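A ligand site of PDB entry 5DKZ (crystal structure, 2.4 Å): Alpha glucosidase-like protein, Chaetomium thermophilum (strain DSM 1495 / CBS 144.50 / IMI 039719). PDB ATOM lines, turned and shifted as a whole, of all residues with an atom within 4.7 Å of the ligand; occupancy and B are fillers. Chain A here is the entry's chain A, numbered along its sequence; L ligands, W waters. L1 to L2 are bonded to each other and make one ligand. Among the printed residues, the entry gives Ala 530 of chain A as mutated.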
ATOM      1  N   HIS A   8      34.165  35.808 -22.784  1.00  0.00           N
ATOM      2  CA  HIS A   8      32.743  35.795 -23.123  1.00  0.00           C
ATOM      3  C   HIS A   8      32.192  37.211 -23.178  1.00  0.00           C
ATOM      4  O   HIS A   8      32.572  38.091 -22.400  1.00  0.00           O
ATOM      5  CB  HIS A   8      31.964  34.965 -22.110  1.00  0.00           C
ATOM      6  CG  HIS A   8      32.212  33.494 -22.217  1.00  0.00           C
ATOM      7  ND1 HIS A   8      33.466  32.934 -22.067  1.00  0.00           N
ATOM      8  CD2 HIS A   8      31.365  32.462 -22.470  1.00  0.00           C
ATOM      9  CE1 HIS A   8      33.383  31.622 -22.229  1.00  0.00           C
ATOM     10  NE2 HIS A   8      32.124  31.318 -22.466  1.00  0.00           N
ATOM     11  N   ASP A 277      24.757  29.533 -22.088  1.00  0.00           N
ATOM     12  CA  ASP A 277      25.889  28.814 -21.529  1.00  0.00           C
ATOM     13  C   ASP A 277      26.854  29.848 -20.963  1.00  0.00           C
ATOM     14  O   ASP A 277      27.623  30.419 -21.704  1.00  0.00           O
ATOM     15  CB  ASP A 277      26.537  27.982 -22.652  1.00  0.00           C
ATOM     16  CG  ASP A 277      27.628  27.047 -22.172  1.00  0.00           C
ATOM     17  OD1 ASP A 277      28.078  27.156 -21.006  1.00  0.00           O
ATOM     18  OD2 ASP A 277      28.076  26.216 -22.985  1.00  0.00           O
ATOM     19  N   PHE A 279      29.798  30.189 -18.910  1.00  0.00           N
ATOM     20  CA  PHE A 279      31.122  29.880 -18.365  1.00  0.00           C
ATOM     21  C   PHE A 279      31.513  30.759 -17.175  1.00  0.00           C
ATOM     22  O   PHE A 279      31.649  31.971 -17.307  1.00  0.00           O
ATOM     23  CB  PHE A 279      32.139  30.081 -19.512  1.00  0.00           C
ATOM     24  CG  PHE A 279      33.555  29.646 -19.195  1.00  0.00           C
ATOM     25  CD1 PHE A 279      33.849  28.322 -18.872  1.00  0.00           C
ATOM     26  CD2 PHE A 279      34.619  30.568 -19.292  1.00  0.00           C
ATOM     27  CE1 PHE A 279      35.162  27.929 -18.634  1.00  0.00           C
ATOM     28  CE2 PHE A 279      35.924  30.176 -19.042  1.00  0.00           C
ATOM     29  CZ  PHE A 279      36.197  28.846 -18.707  1.00  0.00           C
ATOM     30  N   TRP A 389      33.873  15.077 -15.287  1.00  0.00           N
ATOM     31  CA  TRP A 389      34.367  15.107 -16.650  1.00  0.00           C
ATOM     32  C   TRP A 389      35.850  14.685 -16.645  1.00  0.00           C
ATOM     33  O   TRP A 389      36.727  15.537 -16.397  1.00  0.00           O
ATOM     34  CB  TRP A 389      34.216  16.532 -17.186  1.00  0.00           C
ATOM     35  CG  TRP A 389      34.562  16.705 -18.635  1.00  0.00           C
ATOM     36  CD1 TRP A 389      34.723  15.714 -19.562  1.00  0.00           C
ATOM     37  CD2 TRP A 389      34.785  17.940 -19.329  1.00  0.00           C
ATOM     38  NE1 TRP A 389      35.031  16.259 -20.776  1.00  0.00           N
ATOM     39  CE2 TRP A 389      35.064  17.620 -20.664  1.00  0.00           C
ATOM     40  CE3 TRP A 389      34.760  19.286 -18.951  1.00  0.00           C
ATOM     41  CZ2 TRP A 389      35.347  18.607 -21.641  1.00  0.00           C
ATOM     42  CZ3 TRP A 389      35.030  20.266 -19.928  1.00  0.00           C
ATOM     43  CH2 TRP A 389      35.324  19.919 -21.232  1.00  0.00           C
ATOM     44  N   ASP A 417      30.298  11.472 -18.703  1.00  0.00           N
ATOM     45  CA  ASP A 417      30.317  12.666 -19.506  1.00  0.00           C
ATOM     46  C   ASP A 417      30.895  12.351 -20.896  1.00  0.00           C
ATOM     47  O   ASP A 417      31.217  11.218 -21.193  1.00  0.00           O
ATOM     48  CB  ASP A 417      31.177  13.694 -18.761  1.00  0.00           C
ATOM     49  CG  ASP A 417      30.735  15.123 -18.983  1.00  0.00           C
ATOM     50  OD1 ASP A 417      30.139  15.468 -20.037  1.00  0.00           O
ATOM     51  OD2 ASP A 417      31.049  15.922 -18.078  1.00  0.00           O
ATOM     52  N   ILE A 418      31.059  13.389 -21.710  1.00  0.00           N
ATOM     53  CA  ILE A 418      31.103  13.268 -23.183  1.00  0.00           C
ATOM     54  C   ILE A 418      32.246  12.431 -23.762  1.00  0.00           C
ATOM     55  O   ILE A 418      32.110  11.907 -24.898  1.00  0.00           O
ATOM     56  CB  ILE A 418      31.184  14.640 -23.835  1.00  0.00           C
ATOM     57  CG1 ILE A 418      32.389  15.429 -23.273  1.00  0.00           C
ATOM     58  CG2 ILE A 418      29.872  15.386 -23.669  1.00  0.00           C
ATOM     59  CD1 ILE A 418      32.583  16.782 -23.929  1.00  0.00           C
ATOM     60  N   ILE A 454      25.638  11.062 -20.927  1.00  0.00           N
ATOM     61  CA  ILE A 454      25.265  12.327 -21.548  1.00  0.00           C
ATOM     62  C   ILE A 454      24.875  12.180 -23.036  1.00  0.00           C
ATOM     63  O   ILE A 454      25.544  11.478 -23.797  1.00  0.00           O
ATOM     64  CB  ILE A 454      26.371  13.394 -21.347  1.00  0.00           C
ATOM     65  CG1 ILE A 454      25.848  14.791 -21.678  1.00  0.00           C
ATOM     66  CG2 ILE A 454      27.605  13.089 -22.175  1.00  0.00           C
ATOM     67  CD1 ILE A 454      26.672  15.885 -21.036  1.00  0.00           C
ATOM     68  N   TRP A 491      31.035  20.644 -29.205  1.00  0.00           N
ATOM     69  CA  TRP A 491      32.040  19.625 -28.859  1.00  0.00           C
ATOM     70  C   TRP A 491      32.644  18.889 -30.058  1.00  0.00           C
ATOM     71  O   TRP A 491      33.860  18.654 -30.064  1.00  0.00           O
ATOM     72  CB  TRP A 491      31.504  18.558 -27.856  1.00  0.00           C
ATOM     73  CG  TRP A 491      31.161  19.123 -26.503  1.00  0.00           C
ATOM     74  CD1 TRP A 491      29.975  19.010 -25.855  1.00  0.00           C
ATOM     75  CD2 TRP A 491      32.012  19.931 -25.674  1.00  0.00           C
ATOM     76  NE1 TRP A 491      30.050  19.668 -24.654  1.00  0.00           N
ATOM     77  CE2 TRP A 491      31.273  20.250 -24.523  1.00  0.00           C
ATOM     78  CE3 TRP A 491      33.335  20.387 -25.782  1.00  0.00           C
ATOM     79  CZ2 TRP A 491      31.801  21.028 -23.487  1.00  0.00           C
ATOM     80  CZ3 TRP A 491      33.855  21.164 -24.752  1.00  0.00           C
ATOM     81  CH2 TRP A 491      33.083  21.470 -23.624  1.00  0.00           C
ATOM     82  N   TRP A 528      21.390  12.251 -19.341  1.00  0.00           N
ATOM     83  CA  TRP A 528      21.715  13.585 -18.918  1.00  0.00           C
ATOM     84  C   TRP A 528      21.767  14.419 -20.206  1.00  0.00           C
ATOM     85  O   TRP A 528      22.510  14.087 -21.107  1.00  0.00           O
ATOM     86  CB  TRP A 528      23.096  13.510 -18.232  1.00  0.00           C
ATOM     87  CG  TRP A 528      23.813  14.760 -17.972  1.00  0.00           C
ATOM     88  CD1 TRP A 528      23.273  16.010 -17.853  1.00  0.00           C
ATOM     89  CD2 TRP A 528      25.218  14.907 -17.763  1.00  0.00           C
ATOM     90  NE1 TRP A 528      24.276  16.928 -17.608  1.00  0.00           N
ATOM     91  CE2 TRP A 528      25.470  16.280 -17.546  1.00  0.00           C
ATOM     92  CE3 TRP A 528      26.293  14.013 -17.738  1.00  0.00           C
ATOM     93  CZ2 TRP A 528      26.749  16.777 -17.287  1.00  0.00           C
ATOM     94  CZ3 TRP A 528      27.556  14.509 -17.508  1.00  0.00           C
ATOM     95  CH2 TRP A 528      27.780  15.891 -17.268  1.00  0.00           C
ATOM     96  N   ALA A 530      22.737  18.166 -21.493  1.00  0.00           N
ATOM     97  CA  ALA A 530      23.296  19.512 -21.375  1.00  0.00           C
ATOM     98  C   ALA A 530      23.418  20.224 -22.758  1.00  0.00           C
ATOM     99  O   ALA A 530      23.018  19.676 -23.785  1.00  0.00           O
ATOM    100  CB  ALA A 530      24.677  19.406 -20.739  1.00  0.00           C
ATOM    101  N   MET A 531      23.965  21.436 -22.758  1.00  0.00           N
ATOM    102  CA  MET A 531      24.234  22.195 -23.969  1.00  0.00           C
ATOM    103  C   MET A 531      22.978  22.501 -24.727  1.00  0.00           C
ATOM    104  O   MET A 531      23.042  22.874 -25.908  1.00  0.00           O
ATOM    105  CB  MET A 531      25.239  21.468 -24.887  1.00  0.00           C
ATOM    106  CG  MET A 531      26.399  20.795 -24.163  1.00  0.00           C
ATOM    107  SD  MET A 531      27.327  21.978 -23.173  1.00  0.00           S
ATOM    108  CE  MET A 531      28.283  22.840 -24.447  1.00  0.00           C
ATOM    109  N   SER A 535      23.670  25.621 -26.664  1.00  0.00           N
ATOM    110  CA  SER A 535      25.022  26.121 -26.624  1.00  0.00           C
ATOM    111  C   SER A 535      25.652  25.968 -28.002  1.00  0.00           C
ATOM    112  O   SER A 535      25.777  24.850 -28.521  1.00  0.00           O
ATOM    113  CB  SER A 535      25.822  25.356 -25.575  1.00  0.00           C
ATOM    114  OG  SER A 535      27.144  25.854 -25.477  1.00  0.00           O
ATOM    115  N   PHE A 537      29.227  27.274 -29.808  1.00  0.00           N
ATOM    116  CA  PHE A 537      30.499  27.853 -29.387  1.00  0.00           C
ATOM    117  C   PHE A 537      30.847  29.089 -30.201  1.00  0.00           C
ATOM    118  O   PHE A 537      31.288  30.086 -29.661  1.00  0.00           O
ATOM    119  CB  PHE A 537      31.636  26.836 -29.462  1.00  0.00           C
ATOM    120  CG  PHE A 537      31.581  25.739 -28.406  1.00  0.00           C
ATOM    121  CD1 PHE A 537      30.627  25.747 -27.381  1.00  0.00           C
ATOM    122  CD2 PHE A 537      32.487  24.677 -28.452  1.00  0.00           C
ATOM    123  CE1 PHE A 537      30.598  24.733 -26.428  1.00  0.00           C
ATOM    124  CE2 PHE A 537      32.445  23.657 -27.498  1.00  0.00           C
ATOM    125  CZ  PHE A 537      31.505  23.700 -26.476  1.00  0.00           C
ATOM    126  N   ARG A 591      20.090  20.882 -18.349  1.00  0.00           N
ATOM    127  CA  ARG A 591      20.723  22.129 -17.974  1.00  0.00           C
ATOM    128  C   ARG A 591      19.797  23.310 -18.173  1.00  0.00           C
ATOM    129  O   ARG A 591      19.613  24.130 -17.264  1.00  0.00           O
ATOM    130  CB  ARG A 591      22.013  22.346 -18.715  1.00  0.00           C
ATOM    131  CG  ARG A 591      22.868  23.426 -18.048  1.00  0.00           C
ATOM    132  CD  ARG A 591      24.297  23.314 -18.516  1.00  0.00           C
ATOM    133  NE  ARG A 591      24.411  23.859 -19.854  1.00  0.00           N
ATOM    134  CZ  ARG A 591      25.564  24.066 -20.509  1.00  0.00           C
ATOM    135  NH1 ARG A 591      25.516  24.591 -21.707  1.00  0.00           N
ATOM    136  NH2 ARG A 591      26.726  23.777 -19.961  1.00  0.00           N
ATOM    137  N   TRP A 604      20.224  21.128 -12.646  1.00  0.00           N
ATOM    138  CA  TRP A 604      21.256  21.589 -11.792  1.00  0.00           C
ATOM    139  C   TRP A 604      21.690  22.965 -12.267  1.00  0.00           C
ATOM    140  O   TRP A 604      21.339  23.389 -13.370  1.00  0.00           O
ATOM    141  CB  TRP A 604      22.391  20.567 -11.745  1.00  0.00           C
ATOM    142  CG  TRP A 604      23.529  20.775 -12.701  1.00  0.00           C
ATOM    143  CD1 TRP A 604      24.764  21.221 -12.382  1.00  0.00           C
ATOM    144  CD2 TRP A 604      23.557  20.489 -14.100  1.00  0.00           C
ATOM    145  NE1 TRP A 604      25.546  21.278 -13.493  1.00  0.00           N
ATOM    146  CE2 TRP A 604      24.844  20.817 -14.564  1.00  0.00           C
ATOM    147  CE3 TRP A 604      22.610  19.986 -15.002  1.00  0.00           C
ATOM    148  CZ2 TRP A 604      25.220  20.663 -15.898  1.00  0.00           C
ATOM    149  CZ3 TRP A 604      22.981  19.827 -16.313  1.00  0.00           C
ATOM    150  CH2 TRP A 604      24.280  20.176 -16.761  1.00  0.00           C
ATOM    151  N   ASP A 607      27.550  25.386 -14.354  1.00  0.00           N
ATOM    152  CA  ASP A 607      28.967  25.363 -14.041  1.00  0.00           C
ATOM    153  C   ASP A 607      29.305  26.324 -12.916  1.00  0.00           C
ATOM    154  O   ASP A 607      29.772  27.389 -13.144  1.00  0.00           O
ATOM    155  CB  ASP A 607      29.812  25.614 -15.275  1.00  0.00           C
ATOM    156  CG  ASP A 607      29.502  24.645 -16.389  1.00  0.00           C
ATOM    157  OD1 ASP A 607      29.039  23.500 -16.080  1.00  0.00           O
ATOM    158  OD2 ASP A 607      29.718  25.048 -17.559  1.00  0.00           O
ATOM    159  N   PHE A 640      32.113  22.996  -9.704  1.00  0.00           N
ATOM    160  CA  PHE A 640      32.496  22.359 -10.942  1.00  0.00           C
ATOM    161  C   PHE A 640      33.904  22.780 -11.318  1.00  0.00           C
ATOM    162  O   PHE A 640      34.758  21.918 -11.483  1.00  0.00           O
ATOM    163  CB  PHE A 640      31.499  22.675 -12.039  1.00  0.00           C
ATOM    164  CG  PHE A 640      31.864  22.129 -13.404  1.00  0.00           C
ATOM    165  CD1 PHE A 640      31.756  20.782 -13.685  1.00  0.00           C
ATOM    166  CD2 PHE A 640      32.223  22.982 -14.435  1.00  0.00           C
ATOM    167  CE1 PHE A 640      32.060  20.295 -14.951  1.00  0.00           C
ATOM    168  CE2 PHE A 640      32.532  22.502 -15.707  1.00  0.00           C
ATOM    169  CZ  PHE A 640      32.436  21.163 -15.954  1.00  0.00           C
ATOM    170  N   PHE A 641      34.150  24.087 -11.450  1.00  0.00           N
ATOM    171  CA  PHE A 641      35.484  24.606 -11.776  1.00  0.00           C
ATOM    172  C   PHE A 641      36.391  24.634 -10.576  1.00  0.00           C
ATOM    173  O   PHE A 641      36.045  25.221  -9.543  1.00  0.00           O
ATOM    174  CB  PHE A 641      35.439  26.040 -12.324  1.00  0.00           C
ATOM    175  CG  PHE A 641      34.828  26.138 -13.680  1.00  0.00           C
ATOM    176  CD1 PHE A 641      35.485  25.625 -14.801  1.00  0.00           C
ATOM    177  CD2 PHE A 641      33.563  26.732 -13.850  1.00  0.00           C
ATOM    178  CE1 PHE A 641      34.898  25.713 -16.070  1.00  0.00           C
ATOM    179  CE2 PHE A 641      32.984  26.821 -15.112  1.00  0.00           C
ATOM    180  CZ  PHE A 641      33.649  26.308 -16.228  1.00  0.00           C
ATOM    181  N   ARG A 663      24.379  15.525  -6.553  1.00  0.00           N
ATOM    182  CA  ARG A 663      25.399  14.985  -7.425  1.00  0.00           C
ATOM    183  C   ARG A 663      26.705  15.733  -7.206  1.00  0.00           C
ATOM    184  O   ARG A 663      26.730  16.967  -7.185  1.00  0.00           O
ATOM    185  CB  ARG A 663      24.985  15.145  -8.899  1.00  0.00           C
ATOM    186  CG  ARG A 663      26.020  14.708  -9.929  1.00  0.00           C
ATOM    187  CD  ARG A 663      25.571  14.950 -11.356  1.00  0.00           C
ATOM    188  NE  ARG A 663      25.720  16.372 -11.745  1.00  0.00           N
ATOM    189  CZ  ARG A 663      25.862  16.823 -12.983  1.00  0.00           C
ATOM    190  NH1 ARG A 663      25.884  16.001 -14.027  1.00  0.00           N
ATOM    191  NH2 ARG A 663      25.979  18.131 -13.191  1.00  0.00           N
ATOM    192  N   HIS A 665      30.288  16.599  -9.018  1.00  0.00           N
ATOM    193  CA  HIS A 665      30.701  16.737 -10.423  1.00  0.00           C
ATOM    194  C   HIS A 665      31.901  17.676 -10.484  1.00  0.00           C
ATOM    195  O   HIS A 665      32.132  18.465  -9.568  1.00  0.00           O
ATOM    196  CB  HIS A 665      29.520  17.232 -11.285  1.00  0.00           C
ATOM    197  CG  HIS A 665      29.805  17.321 -12.752  1.00  0.00           C
ATOM    198  ND1 HIS A 665      30.646  16.462 -13.408  1.00  0.00           N
ATOM    199  CD2 HIS A 665      29.342  18.179 -13.689  1.00  0.00           C
ATOM    200  CE1 HIS A 665      30.731  16.807 -14.686  1.00  0.00           C
ATOM    201  NE2 HIS A 665      29.938  17.855 -14.881  1.00  0.00           N
ATOM    202  N   HIS A 667      35.152  19.531 -13.210  1.00  0.00           N
ATOM    203  CA  HIS A 667      35.620  19.949 -14.524  1.00  0.00           C
ATOM    204  C   HIS A 667      36.871  19.126 -14.929  1.00  0.00           C
ATOM    205  O   HIS A 667      37.551  18.538 -14.072  1.00  0.00           O
ATOM    206  CB  HIS A 667      35.885  21.458 -14.494  1.00  0.00           C
ATOM    207  CG  HIS A 667      36.594  22.017 -15.681  1.00  0.00           C
ATOM    208  ND1 HIS A 667      35.945  22.443 -16.817  1.00  0.00           N
ATOM    209  CD2 HIS A 667      37.912  22.296 -15.882  1.00  0.00           C
ATOM    210  CE1 HIS A 667      36.819  22.946 -17.668  1.00  0.00           C
ATOM    211  NE2 HIS A 667      38.021  22.854 -17.128  1.00  0.00           N
HETATM  212  C1  LIG L   1      33.247  24.534 -20.101  1.00  0.00           C
HETATM  213  C2  LIG L   1      32.162  23.696 -19.414  1.00  0.00           C
HETATM  214  C3  LIG L   1      30.873  23.391 -20.207  1.00  0.00           C
HETATM  215  C4  LIG L   1      30.476  24.600 -21.050  1.00  0.00           C
HETATM  216  C5  LIG L   1      31.664  25.192 -21.858  1.00  0.00           C
HETATM  217  C6  LIG L   1      31.297  26.467 -22.642  1.00  0.00           C
HETATM  218  O1  LIG L   1      34.158  23.679 -20.768  1.00  0.00           O
HETATM  219  O2  LIG L   1      32.732  22.456 -19.047  1.00  0.00           O
HETATM  220  O3  LIG L   1      30.153  22.513 -19.462  1.00  0.00           O
HETATM  221  O4  LIG L   1      29.374  24.243 -21.878  1.00  0.00           O
HETATM  222  O5  LIG L   1      32.749  25.537 -21.007  1.00  0.00           O
HETATM  223  O6  LIG L   1      30.661  27.402 -21.774  1.00  0.00           O
HETATM  224  C1  LG2 L   2      29.257  21.508 -19.885  1.00  0.00           C
HETATM  225  C2  LG2 L   2      28.386  20.996 -18.732  1.00  0.00           C
HETATM  226  C3  LG2 L   2      29.210  20.185 -17.731  1.00  0.00           C
HETATM  227  C4  LG2 L   2      29.901  19.029 -18.467  1.00  0.00           C
HETATM  228  C5  LG2 L   2      30.674  19.540 -19.691  1.00  0.00           C
HETATM  229  C6  LG2 L   2      31.183  18.391 -20.551  1.00  0.00           C
HETATM  230  O1  LG2 L   2      27.754  22.065 -18.093  1.00  0.00           O
HETATM  231  O2  LG2 L   2      28.404  19.714 -16.667  1.00  0.00           O
HETATM  232  O3  LG2 L   2      30.794  18.385 -17.581  1.00  0.00           O
HETATM  233  O4  LG2 L   2      29.957  20.430 -20.516  1.00  0.00           O
HETATM  234  O5  LG2 L   2      30.119  17.800 -21.241  1.00  0.00           O
HETATM  235  O   HOH W   1      28.321  21.468 -14.459  1.00  0.00           O
HETATM  236  O   HOH W   2      28.109  18.773 -22.567  1.00  0.00           O
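An oxygen (O3) of LG2 L2 lies within hydrogen-bond range of the side-chain carboxylate of Asp 417 (2.5 Å).
OD2 of Asp 277 is in hydrogen-bond range of O4 of LIG L1 (2.6 Å).
The guanidinium group (NH2) of Arg 591 sits at hydrogen-bond distance from an oxygen (O1) of LG2 L2.
An oxygen (O1) of LG2 L2 is in hydrogen-bond range of the side-chain carboxylate (OD1) of Asp 607 (2.8 Å).
NE2 of His 665 lies within hydrogen-bond range of O3 of LG2 L2, at 2.9 Å.
SD of Met 531 lies close to O4 of LIG L1, 3.3 Å away.
The side-chain carboxylate of Asp 277 lies within salt-bridge range of the guanidinium group of Arg 591 (3.3 Å).
The side-chain hydroxyl (OG) of Ser 535 is in hydrogen-bond range of the side-chain carboxylate (OD2) of Asp 277 (2.7 Å).
NH1 of Arg 591 lies within hydrogen-bond range of SD of Met 531 (3.5 Å).
The backbone carbonyl oxygen of Phe 640 sits at hydrogen-bond distance from the backbone NH of His 667.
CD1 of Phe 279 touches O5 of LIG L1 (3.7 Å).
CZ3 of Trp 389 touches O2 of LIG L1 (3.3 Å).
CG2 of Ile 418 touches O5 of LG2 L2 (3.4 Å).
CD1 of Ile 454 touches O5 of LG2 L2, at 3.9 Å.
Trp 491 touches the ligand.
CZ2 of Trp 528 touches O2 of LG2 L2, at 3.4 Å.
CZ2 of Trp 604 touches O2 of LG2 L2 (3.4 Å).
Phe 640 touches the ligand.
ND1 of His 667 touches O2 of LIG L1 (3.9 Å).
Hydrophobic or aromatic side chains within 4 Å of the ligand: Phe 279, Trp 389, Ile 418, Ile 454, Trp 491, Trp 528, Met 531, Trp 604, Phe 640 and His 665.
Within 4 Å of the ligand: Asp 277, Phe 279, Trp 389, Asp 417, Ile 418, Ile 454, Trp 491, Trp 528, Met 531, Arg 591, Trp 604, Asp 607, Phe 640, His 665 and His 667.
The nearest printed residue that does not touch the ligand is Phe 537 (4.2 Å).
Water W2 lies within hydrogen-bond range of an oxygen (O5) of LG2 L2, the indole nitrogen of Trp 491 and the side-chain sulfur of Met 531.
Water W1 lies within hydrogen-bond range of the side-chain carboxylate of Asp 607, an oxygen (O2) of LG2 L2 and the indole nitrogen of Trp 604.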
